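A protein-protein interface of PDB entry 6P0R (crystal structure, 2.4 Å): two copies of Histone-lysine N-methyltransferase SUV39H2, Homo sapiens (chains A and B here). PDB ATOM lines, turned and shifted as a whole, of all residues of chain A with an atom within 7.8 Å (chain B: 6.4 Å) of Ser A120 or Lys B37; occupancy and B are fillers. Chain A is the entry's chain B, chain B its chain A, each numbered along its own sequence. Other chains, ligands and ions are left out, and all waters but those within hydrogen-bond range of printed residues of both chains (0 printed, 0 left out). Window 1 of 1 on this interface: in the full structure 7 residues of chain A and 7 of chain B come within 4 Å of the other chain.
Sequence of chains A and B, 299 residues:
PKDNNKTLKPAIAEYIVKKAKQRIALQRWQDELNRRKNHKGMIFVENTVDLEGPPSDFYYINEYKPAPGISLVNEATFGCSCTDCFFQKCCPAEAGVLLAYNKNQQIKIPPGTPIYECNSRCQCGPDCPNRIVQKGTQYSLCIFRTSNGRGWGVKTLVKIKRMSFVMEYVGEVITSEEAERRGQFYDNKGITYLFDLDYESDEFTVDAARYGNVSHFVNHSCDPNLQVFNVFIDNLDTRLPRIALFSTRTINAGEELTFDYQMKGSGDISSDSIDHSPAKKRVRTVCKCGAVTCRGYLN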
ATOM      1  N   THR A  77     -27.856  -2.029  -3.161  1.00  0.00           N
ATOM      2  CA  THR A  77     -26.687  -2.784  -3.641  1.00  0.00           C
ATOM      3  C   THR A  77     -27.024  -3.918  -4.630  1.00  0.00           C
ATOM      4  O   THR A  77     -28.163  -4.404  -4.708  1.00  0.00           O
ATOM      5  CB  THR A  77     -25.878  -3.388  -2.457  1.00  0.00           C
ATOM      6  OG1 THR A  77     -26.744  -3.606  -1.342  1.00  0.00           O
ATOM      7  CG2 THR A  77     -24.733  -2.451  -2.028  1.00  0.00           C
ATOM      8  N   PHE A  78     -25.993  -4.308  -5.379  1.00  0.00           N
ATOM      9  CA  PHE A  78     -26.039  -5.401  -6.345  1.00  0.00           C
ATOM     10  C   PHE A  78     -24.604  -5.840  -6.616  1.00  0.00           C
ATOM     11  O   PHE A  78     -23.710  -5.002  -6.683  1.00  0.00           O
ATOM     12  CB  PHE A  78     -26.691  -4.932  -7.653  1.00  0.00           C
ATOM     13  CG  PHE A  78     -26.352  -5.788  -8.845  1.00  0.00           C
ATOM     14  CD1 PHE A  78     -26.995  -6.992  -9.045  1.00  0.00           C
ATOM     15  CD2 PHE A  78     -25.360  -5.395  -9.755  1.00  0.00           C
ATOM     16  CE1 PHE A  78     -26.689  -7.796 -10.136  1.00  0.00           C
ATOM     17  CE2 PHE A  78     -25.041  -6.195 -10.844  1.00  0.00           C
ATOM     18  CZ  PHE A  78     -25.712  -7.401 -11.040  1.00  0.00           C
ATOM     19  N   GLY A  79     -24.396  -7.142  -6.760  1.00  0.00           N
ATOM     20  CA  GLY A  79     -23.114  -7.703  -7.205  1.00  0.00           C
ATOM     21  C   GLY A  79     -23.320  -8.635  -8.390  1.00  0.00           C
ATOM     22  O   GLY A  79     -24.341  -9.317  -8.472  1.00  0.00           O
ATOM     23  N   GLU A 117     -17.685  -0.197 -11.391  1.00  0.00           N
ATOM     24  CA  GLU A 117     -16.721  -1.201 -11.022  1.00  0.00           C
ATOM     25  C   GLU A 117     -17.399  -2.347 -10.268  1.00  0.00           C
ATOM     26  O   GLU A 117     -18.480  -2.200  -9.699  1.00  0.00           O
ATOM     27  CB  GLU A 117     -15.592  -0.590 -10.168  1.00  0.00           C
ATOM     28  CG  GLU A 117     -14.765   0.459 -10.921  1.00  0.00           C
ATOM     29  CD  GLU A 117     -13.327   0.597 -10.433  1.00  0.00           C
ATOM     30  OE1 GLU A 117     -12.995   0.118  -9.327  1.00  0.00           O
ATOM     31  OE2 GLU A 117     -12.508   1.191 -11.174  1.00  0.00           O
ATOM     32  N   CYS A 118     -16.750  -3.492 -10.291  1.00  0.00           N
ATOM     33  CA  CYS A 118     -17.131  -4.594  -9.443  1.00  0.00           C
ATOM     34  C   CYS A 118     -16.876  -4.193  -7.994  1.00  0.00           C
ATOM     35  O   CYS A 118     -16.022  -3.344  -7.713  1.00  0.00           O
ATOM     36  CB  CYS A 118     -16.362  -5.830  -9.828  1.00  0.00           C
ATOM     37  SG  CYS A 118     -17.051  -6.634 -11.273  1.00  0.00           S
ATOM     38  N   ASN A 119     -17.641  -4.782  -7.089  1.00  0.00           N
ATOM     39  CA  ASN A 119     -17.743  -4.293  -5.727  1.00  0.00           C
ATOM     40  C   ASN A 119     -17.725  -5.446  -4.706  1.00  0.00           C
ATOM     41  O   ASN A 119     -17.476  -6.606  -5.066  1.00  0.00           O
ATOM     42  CB  ASN A 119     -18.994  -3.382  -5.606  1.00  0.00           C
ATOM     43  CG  ASN A 119     -20.306  -4.136  -5.754  1.00  0.00           C
ATOM     44  OD1 ASN A 119     -20.653  -4.969  -4.919  1.00  0.00           O
ATOM     45  ND2 ASN A 119     -21.062  -3.817  -6.807  1.00  0.00           N
ATOM     46  N   SER A 120     -17.959  -5.126  -3.438  1.00  0.00           N
ATOM     47  CA  SER A 120     -17.851  -6.110  -2.362  1.00  0.00           C
ATOM     48  C   SER A 120     -18.918  -7.221  -2.389  1.00  0.00           C
ATOM     49  O   SER A 120     -18.711  -8.272  -1.795  1.00  0.00           O
ATOM     50  CB  SER A 120     -17.839  -5.404  -1.000  1.00  0.00           C
ATOM     51  OG  SER A 120     -18.832  -4.418  -0.940  1.00  0.00           O
ATOM     52  N   ARG A 121     -20.041  -6.988  -3.076  1.00  0.00           N
ATOM     53  CA  ARG A 121     -21.090  -8.018  -3.274  1.00  0.00           C
ATOM     54  C   ARG A 121     -20.842  -8.953  -4.485  1.00  0.00           C
ATOM     55  O   ARG A 121     -21.582  -9.914  -4.677  1.00  0.00           O
ATOM     56  CB  ARG A 121     -22.472  -7.350  -3.429  1.00  0.00           C
ATOM     57  CG  ARG A 121     -22.969  -6.629  -2.181  1.00  0.00           C
ATOM     58  N   CYS A 122     -19.828  -8.655  -5.306  1.00  0.00           N
ATOM     59  CA  CYS A 122     -19.565  -9.433  -6.526  1.00  0.00           C
ATOM     60  C   CYS A 122     -18.856 -10.757  -6.180  1.00  0.00           C
ATOM     61  O   CYS A 122     -18.273 -10.905  -5.097  1.00  0.00           O
ATOM     62  CB  CYS A 122     -18.701  -8.633  -7.507  1.00  0.00           C
ATOM     63  SG  CYS A 122     -19.403  -7.103  -8.171  1.00  0.00           S
ATOM     64  N   GLN A 123     -18.914 -11.710  -7.106  1.00  0.00           N
ATOM     65  CA  GLN A 123     -18.308 -13.028  -6.906  1.00  0.00           C
ATOM     66  C   GLN A 123     -16.831 -13.095  -7.295  1.00  0.00           C
ATOM     67  O   GLN A 123     -16.181 -14.100  -7.040  1.00  0.00           O
ATOM     68  CB  GLN A 123     -19.099 -14.098  -7.666  1.00  0.00           C
ATOM     69  CG  GLN A 123     -20.531 -14.256  -7.180  1.00  0.00           C
ATOM     70  CD  GLN A 123     -20.616 -14.575  -5.692  1.00  0.00           C
ATOM     71  OE1 GLN A 123     -20.148 -15.628  -5.242  1.00  0.00           O
ATOM     72  NE2 GLN A 123     -21.200 -13.663  -4.920  1.00  0.00           N
ATOM     73  N   CYS A 124     -16.314 -12.034  -7.906  1.00  0.00           N
ATOM     74  CA  CYS A 124     -14.917 -11.963  -8.331  1.00  0.00           C
ATOM     75  C   CYS A 124     -14.017 -11.414  -7.243  1.00  0.00           C
ATOM     76  O   CYS A 124     -14.468 -10.668  -6.360  1.00  0.00           O
ATOM     77  CB  CYS A 124     -14.802 -11.085  -9.573  1.00  0.00           C
ATOM     78  SG  CYS A 124     -15.415  -9.401  -9.331  1.00  0.00           S
ATOM     79  N   ARG A 131     -11.759  -3.748 -11.529  1.00  0.00           N
ATOM     80  CA  ARG A 131     -11.383  -3.150 -10.240  1.00  0.00           C
ATOM     81  C   ARG A 131     -10.100  -2.328 -10.398  1.00  0.00           C
ATOM     82  O   ARG A 131      -8.998  -2.832 -10.129  1.00  0.00           O
ATOM     83  CB  ARG A 131     -11.162  -4.247  -9.187  1.00  0.00           C
ATOM     84  CG  ARG A 131     -12.388  -5.082  -8.867  1.00  0.00           C
ATOM     85  CD  ARG A 131     -12.045  -6.140  -7.830  1.00  0.00           C
ATOM     86  NE  ARG A 131     -13.171  -7.036  -7.535  1.00  0.00           N
ATOM     87  CZ  ARG A 131     -14.205  -6.743  -6.738  1.00  0.00           C
ATOM     88  NH1 ARG A 131     -14.305  -5.560  -6.155  1.00  0.00           N
ATOM     89  NH2 ARG A 131     -15.161  -7.641  -6.548  1.00  0.00           N
ATOM     90  N   GLN A 134     -10.874   1.571  -7.360  1.00  0.00           N
ATOM     91  CA  GLN A 134     -10.924   1.091  -5.976  1.00  0.00           C
ATOM     92  C   GLN A 134      -9.567   0.642  -5.410  1.00  0.00           C
ATOM     93  O   GLN A 134      -9.366   0.696  -4.206  1.00  0.00           O
ATOM     94  CB  GLN A 134     -11.948  -0.047  -5.846  1.00  0.00           C
ATOM     95  CG  GLN A 134     -11.559  -1.336  -6.556  1.00  0.00           C
ATOM     96  CD  GLN A 134     -12.729  -2.264  -6.729  1.00  0.00           C
ATOM     97  OE1 GLN A 134     -12.816  -3.292  -6.058  1.00  0.00           O
ATOM     98  NE2 GLN A 134     -13.650  -1.905  -7.622  1.00  0.00           N
ATOM     99  N   ILE A 233     -18.947   2.114  -7.150  1.00  0.00           N
ATOM    100  CA  ILE A 233     -18.400   0.856  -6.649  1.00  0.00           C
ATOM    101  C   ILE A 233     -19.471   0.252  -5.713  1.00  0.00           C
ATOM    102  O   ILE A 233     -20.371  -0.418  -6.192  1.00  0.00           O
ATOM    103  CB  ILE A 233     -17.013   1.076  -5.965  1.00  0.00           C
ATOM    104  CG1 ILE A 233     -16.008   1.653  -6.959  1.00  0.00           C
ATOM    105  CG2 ILE A 233     -16.464  -0.228  -5.408  1.00  0.00           C
ATOM    106  CD1 ILE A 233     -14.979   2.554  -6.319  1.00  0.00           C
ATOM    107  N   ASP A 234     -19.411   0.525  -4.402  1.00  0.00           N
ATOM    108  CA  ASP A 234     -20.429  -0.005  -3.463  1.00  0.00           C
ATOM    109  C   ASP A 234     -21.728   0.811  -3.547  1.00  0.00           C
ATOM    110  O   ASP A 234     -22.818   0.250  -3.541  1.00  0.00           O
ATOM    111  CB  ASP A 234     -19.896  -0.041  -2.011  1.00  0.00           C
ATOM    112  CG  ASP A 234     -19.023  -1.270  -1.722  1.00  0.00           C
ATOM    113  OD1 ASP A 234     -19.141  -2.289  -2.429  1.00  0.00           O
ATOM    114  OD2 ASP A 234     -18.222  -1.216  -0.770  1.00  0.00           O
ATOM    115  N   ASN A 235     -21.589   2.128  -3.630  1.00  0.00           N
ATOM    116  CA  ASN A 235     -22.716   3.024  -3.831  1.00  0.00           C
ATOM    117  C   ASN A 235     -23.246   2.974  -5.263  1.00  0.00           C
ATOM    118  O   ASN A 235     -22.495   3.195  -6.208  1.00  0.00           O
ATOM    119  CB  ASN A 235     -22.301   4.461  -3.544  1.00  0.00           C
ATOM    120  CG  ASN A 235     -23.402   5.436  -3.856  1.00  0.00           C
ATOM    121  OD1 ASN A 235     -24.502   5.325  -3.310  1.00  0.00           O
ATOM    122  ND2 ASN A 235     -23.137   6.375  -4.775  1.00  0.00           N
ATOM    123  N   ASP B  31     -20.441  -1.011   6.175  1.00  0.00           N
ATOM    124  CA  ASP B  31     -20.174  -0.446   4.838  1.00  0.00           C
ATOM    125  C   ASP B  31     -18.716   0.012   4.672  1.00  0.00           C
ATOM    126  O   ASP B  31     -18.119  -0.192   3.614  1.00  0.00           O
ATOM    127  CB  ASP B  31     -21.123   0.731   4.540  1.00  0.00           C
ATOM    128  CG  ASP B  31     -22.565   0.283   4.205  1.00  0.00           C
ATOM    129  OD1 ASP B  31     -22.865  -0.941   4.165  1.00  0.00           O
ATOM    130  OD2 ASP B  31     -23.406   1.178   3.966  1.00  0.00           O
ATOM    131  N   GLU B  32     -18.158   0.636   5.710  1.00  0.00           N
ATOM    132  CA  GLU B  32     -16.737   1.016   5.721  1.00  0.00           C
ATOM    133  C   GLU B  32     -15.821  -0.210   5.649  1.00  0.00           C
ATOM    134  O   GLU B  32     -14.826  -0.191   4.919  1.00  0.00           O
ATOM    135  CB  GLU B  32     -16.401   1.851   6.964  1.00  0.00           C
ATOM    136  CG  GLU B  32     -14.945   2.297   7.052  1.00  0.00           C
ATOM    137  N   LEU B  33     -16.162  -1.267   6.396  1.00  0.00           N
ATOM    138  CA  LEU B  33     -15.411  -2.532   6.352  1.00  0.00           C
ATOM    139  C   LEU B  33     -15.406  -3.150   4.948  1.00  0.00           C
ATOM    140  O   LEU B  33     -14.357  -3.623   4.483  1.00  0.00           O
ATOM    141  CB  LEU B  33     -15.965  -3.565   7.368  1.00  0.00           C
ATOM    142  CG  LEU B  33     -15.709  -3.380   8.868  1.00  0.00           C
ATOM    143  CD1 LEU B  33     -16.305  -4.559   9.616  1.00  0.00           C
ATOM    144  CD2 LEU B  33     -14.231  -3.256   9.171  1.00  0.00           C
ATOM    145  N   ASN B  34     -16.563  -3.154   4.288  1.00  0.00           N
ATOM    146  CA  ASN B  34     -16.675  -3.724   2.937  1.00  0.00           C
ATOM    147  C   ASN B  34     -16.017  -2.841   1.861  1.00  0.00           C
ATOM    148  O   ASN B  34     -15.705  -3.331   0.771  1.00  0.00           O
ATOM    149  CB  ASN B  34     -18.134  -4.007   2.573  1.00  0.00           C
ATOM    150  CG  ASN B  34     -18.707  -5.178   3.347  1.00  0.00           C
ATOM    151  OD1 ASN B  34     -18.215  -6.301   3.241  1.00  0.00           O
ATOM    152  ND2 ASN B  34     -19.755  -4.921   4.135  1.00  0.00           N
ATOM    153  N   ARG B  35     -15.807  -1.554   2.163  1.00  0.00           N
ATOM    154  CA  ARG B  35     -14.997  -0.677   1.292  1.00  0.00           C
ATOM    155  C   ARG B  35     -13.492  -0.951   1.443  1.00  0.00           C
ATOM    156  O   ARG B  35     -12.792  -1.024   0.446  1.00  0.00           O
ATOM    157  CB  ARG B  35     -15.324   0.820   1.518  1.00  0.00           C
ATOM    158  CG  ARG B  35     -16.195   1.429   0.412  1.00  0.00           C
ATOM    159  CD  ARG B  35     -16.984   2.666   0.848  1.00  0.00           C
ATOM    160  NE  ARG B  35     -16.219   3.530   1.762  1.00  0.00           N
ATOM    161  CZ  ARG B  35     -16.594   3.898   3.002  1.00  0.00           C
ATOM    162  NH1 ARG B  35     -15.777   4.680   3.722  1.00  0.00           N
ATOM    163  NH2 ARG B  35     -17.766   3.515   3.534  1.00  0.00           N
ATOM    164  N   ARG B  36     -13.006  -1.109   2.681  1.00  0.00           N
ATOM    165  CA  ARG B  36     -11.568  -1.380   2.924  1.00  0.00           C
ATOM    166  C   ARG B  36     -11.124  -2.743   2.385  1.00  0.00           C
ATOM    167  O   ARG B  36     -10.076  -2.848   1.757  1.00  0.00           O
ATOM    168  CB  ARG B  36     -11.229  -1.324   4.420  1.00  0.00           C
ATOM    169  CG  ARG B  36     -11.319   0.051   5.068  1.00  0.00           C
ATOM    170  CD  ARG B  36     -10.261   1.024   4.562  1.00  0.00           C
ATOM    171  NE  ARG B  36     -10.872   2.115   3.794  1.00  0.00           N
ATOM    172  CZ  ARG B  36     -11.476   3.195   4.319  1.00  0.00           C
ATOM    173  NH1 ARG B  36     -11.561   3.374   5.647  1.00  0.00           N
ATOM    174  NH2 ARG B  36     -11.995   4.115   3.501  1.00  0.00           N
ATOM    175  N   LYS B  37     -11.914  -3.781   2.656  1.00  0.00           N
ATOM    176  CA  LYS B  37     -11.553  -5.148   2.263  1.00  0.00           C
ATOM    177  C   LYS B  37     -11.505  -5.328   0.749  1.00  0.00           C
ATOM    178  O   LYS B  37     -12.325  -4.765   0.030  1.00  0.00           O
ATOM    179  CB  LYS B  37     -12.493  -6.185   2.910  1.00  0.00           C
ATOM    180  CG  LYS B  37     -13.933  -6.201   2.383  1.00  0.00           C
ATOM    181  CD  LYS B  37     -14.202  -7.347   1.407  1.00  0.00           C
ATOM    182  CE  LYS B  37     -15.520  -7.134   0.674  1.00  0.00           C
ATOM    183  NZ  LYS B  37     -16.044  -8.361  -0.007  1.00  0.00           N
ATOM    184  N   ASN B  38     -10.524  -6.111   0.289  1.00  0.00           N
ATOM    185  CA  ASN B  38     -10.302  -6.360  -1.148  1.00  0.00           C
ATOM    186  C   ASN B  38     -10.711  -7.788  -1.640  1.00  0.00           C
ATOM    187  O   ASN B  38     -10.776  -8.018  -2.839  1.00  0.00           O
ATOM    188  CB  ASN B  38      -8.827  -6.058  -1.521  1.00  0.00           C
ATOM    189  CG  ASN B  38      -7.839  -7.082  -0.950  1.00  0.00           C
ATOM    190  OD1 ASN B  38      -8.174  -7.864  -0.059  1.00  0.00           O
ATOM    191  ND2 ASN B  38      -6.610  -7.069  -1.465  1.00  0.00           N
ATOM    192  N   HIS B  39     -10.967  -8.723  -0.717  1.00  0.00           N
ATOM    193  CA  HIS B  39     -11.349 -10.110  -1.085  1.00  0.00           C
ATOM    194  C   HIS B  39     -12.846 -10.263  -1.497  1.00  0.00           C
ATOM    195  O   HIS B  39     -13.639  -9.322  -1.369  1.00  0.00           O
ATOM    196  CB  HIS B  39     -10.992 -11.083   0.060  1.00  0.00           C
ATOM    197  CG  HIS B  39     -11.814 -10.901   1.303  1.00  0.00           C
ATOM    198  ND1 HIS B  39     -11.331 -10.278   2.432  1.00  0.00           N
ATOM    199  CD2 HIS B  39     -13.081 -11.274   1.594  1.00  0.00           C
ATOM    200  CE1 HIS B  39     -12.271 -10.267   3.363  1.00  0.00           C
ATOM    201  NE2 HIS B  39     -13.340 -10.872   2.881  1.00  0.00           N
ATOM    202  N   LYS B  40     -13.200 -11.465  -1.975  1.00  0.00           N
ATOM    203  CA  LYS B  40     -14.577 -11.793  -2.431  1.00  0.00           C
ATOM    204  C   LYS B  40     -15.599 -11.774  -1.289  1.00  0.00           C
ATOM    205  O   LYS B  40     -16.547 -10.985  -1.308  1.00  0.00           O
ATOM    206  CB  LYS B  40     -14.606 -13.190  -3.114  1.00  0.00           C
ATOM    207  CG  LYS B  40     -16.009 -13.675  -3.539  1.00  0.00           C
ATOM    208  CD  LYS B  40     -16.264 -15.170  -3.272  1.00  0.00           C
ATOM    209  CE  LYS B  40     -16.081 -16.024  -4.519  1.00  0.00           C
ATOM    210  N   GLY B  41     -15.413 -12.675  -0.324  1.00  0.00           N
ATOM    211  CA  GLY B  41     -16.335 -12.843   0.806  1.00  0.00           C
ATOM    212  C   GLY B  41     -16.807 -11.547   1.451  1.00  0.00           C
ATOM    213  O   GLY B  41     -16.014 -10.629   1.692  1.00  0.00           O
ATOM    214  N   MET B  42     -18.109 -11.473   1.719  1.00  0.00           N
ATOM    215  CA  MET B  42     -18.699 -10.301   2.368  1.00  0.00           C
ATOM    216  C   MET B  42     -18.368 -10.281   3.859  1.00  0.00           C
ATOM    217  O   MET B  42     -17.992 -11.309   4.443  1.00  0.00           O
ATOM    218  CB  MET B  42     -20.215 -10.283   2.167  1.00  0.00           C
ATOM    219  CG  MET B  42     -20.639  -9.767   0.805  1.00  0.00           C
ATOM    220  SD  MET B  42     -20.887  -7.981   0.840  1.00  0.00           S
ATOM    221  CE  MET B  42     -22.662  -7.879   1.115  1.00  0.00           C
ATOM    222  N   ILE B  43     -18.481  -9.094   4.452  1.00  0.00           N
ATOM    223  CA  ILE B  43     -18.349  -8.903   5.896  1.00  0.00           C
ATOM    224  C   ILE B  43     -19.655  -8.276   6.399  1.00  0.00           C
ATOM    225  O   ILE B  43     -20.077  -7.248   5.886  1.00  0.00           O
ATOM    226  CB  ILE B  43     -17.162  -7.996   6.244  1.00  0.00           C
ATOM    227  CG1 ILE B  43     -15.876  -8.553   5.631  1.00  0.00           C
ATOM    228  CG2 ILE B  43     -16.998  -7.878   7.756  1.00  0.00           C
ATOM    229  CD1 ILE B  43     -14.661  -7.678   5.851  1.00  0.00           C
ATOM    230  N   TYR B  60      -9.136  -1.319   9.191  1.00  0.00           N
ATOM    231  CA  TYR B  60      -9.074  -2.566   8.394  1.00  0.00           C
ATOM    232  C   TYR B  60      -7.962  -2.511   7.348  1.00  0.00           C
ATOM    233  O   TYR B  60      -7.867  -1.541   6.594  1.00  0.00           O
ATOM    234  CB  TYR B  60     -10.410  -2.850   7.706  1.00  0.00           C
ATOM    235  CG  TYR B  60     -10.518  -4.252   7.110  1.00  0.00           C
ATOM    236  CD1 TYR B  60      -9.995  -4.543   5.843  1.00  0.00           C
ATOM    237  CD2 TYR B  60     -11.146  -5.280   7.806  1.00  0.00           C
ATOM    238  CE1 TYR B  60     -10.092  -5.821   5.302  1.00  0.00           C
ATOM    239  CE2 TYR B  60     -11.249  -6.561   7.269  1.00  0.00           C
ATOM    240  CZ  TYR B  60     -10.719  -6.828   6.018  1.00  0.00           C
ATOM    241  OH  TYR B  60     -10.808  -8.095   5.478  1.00  0.00           O
ATOM    242  N   ASN B  62      -5.729  -5.167   4.388  1.00  0.00           N
ATOM    243  CA  ASN B  62      -5.741  -6.429   3.633  1.00  0.00           C
ATOM    244  C   ASN B  62      -4.412  -7.169   3.694  1.00  0.00           C
ATOM    245  O   ASN B  62      -4.358  -8.357   3.377  1.00  0.00           O
ATOM    246  CB  ASN B  62      -6.081  -6.170   2.175  1.00  0.00           C
ATOM    247  CG  ASN B  62      -7.416  -5.502   2.006  1.00  0.00           C
ATOM    248  OD1 ASN B  62      -8.399  -5.954   2.552  1.00  0.00           O
ATOM    249  ND2 ASN B  62      -7.459  -4.427   1.232  1.00  0.00           N
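O of Ser A120 lies close to SD of Met B42, 3.4 Å away.
The backbone carbonyl oxygen (O) of Ser A120 is in hydrogen-bond range of the side-chain amino group (NZ) of Lys B37, at 3.2 Å.
The side-chain carboxylate of Asp A234 is in hydrogen-bond range of the side-chain hydroxyl of Ser A120 (2.6 Å).
The backbone carbonyl oxygen (O) of His B39 is in hydrogen-bond range of the side-chain amino group (NZ) of Lys B37, at 2.9 Å.
SG of Cys A122 lies close to N of Asn A119, 3.1 Å away.
OD1 of Asn A119 is in hydrogen-bond range of N of Arg A121, at 2.8 Å.
The side-chain amide nitrogen (ND2) of Asn B34 lies within hydrogen-bond range of the backbone carbonyl oxygen (O) of Ile B43 (2.9 Å).
The backbone carbonyl oxygen of Gly B41 lies within hydrogen-bond range of the side-chain amino group of Lys B37, at 2.8 Å.
Among the printed residues, merely in contact across the chains: Gln A123 with Lys B40, Ser A120 with Asn B34, Ser A120 with Lys B40, Asp A234 with Arg B35, Arg A121 with Met B42, Asp A234 with Asn B34 and Cys A122 with Lys B40.
Ser A120 touches four residues of chain B.
Lys B37 touches one residue of chain A.
Of the printed residues of chain A, Arg B35 touches Asp A234 (3.5 Å).
Printed residues of chain B within 4 Å of Gln A123: Lys B40.
Of the printed residues of chain A, Lys B40 touches Ser A120, Cys A122 and Gln A123.
The nearest residue of chain B that does not touch Ser A120 is Gly B41 (5.0 Å).
The nearest residue of chain A that does not touch Lys B37 is Arg A121 (5.2 Å).
The nearest printed residue of chain B that does not touch Gln A123 is Gly B41 (6.9 Å).
Of the 16 printed residues of chain A, 5 touch a printed residue of chain B.
Printed residues of chain A that touch a printed residue of chain B: Ser A120, Arg A121, Cys A122, Gln A123 and Asp A234.
No position is printed for both chains.
Of the 9 pairs that touch across the chains among the printed residues, none has its exchanged pair printed and touching as well.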
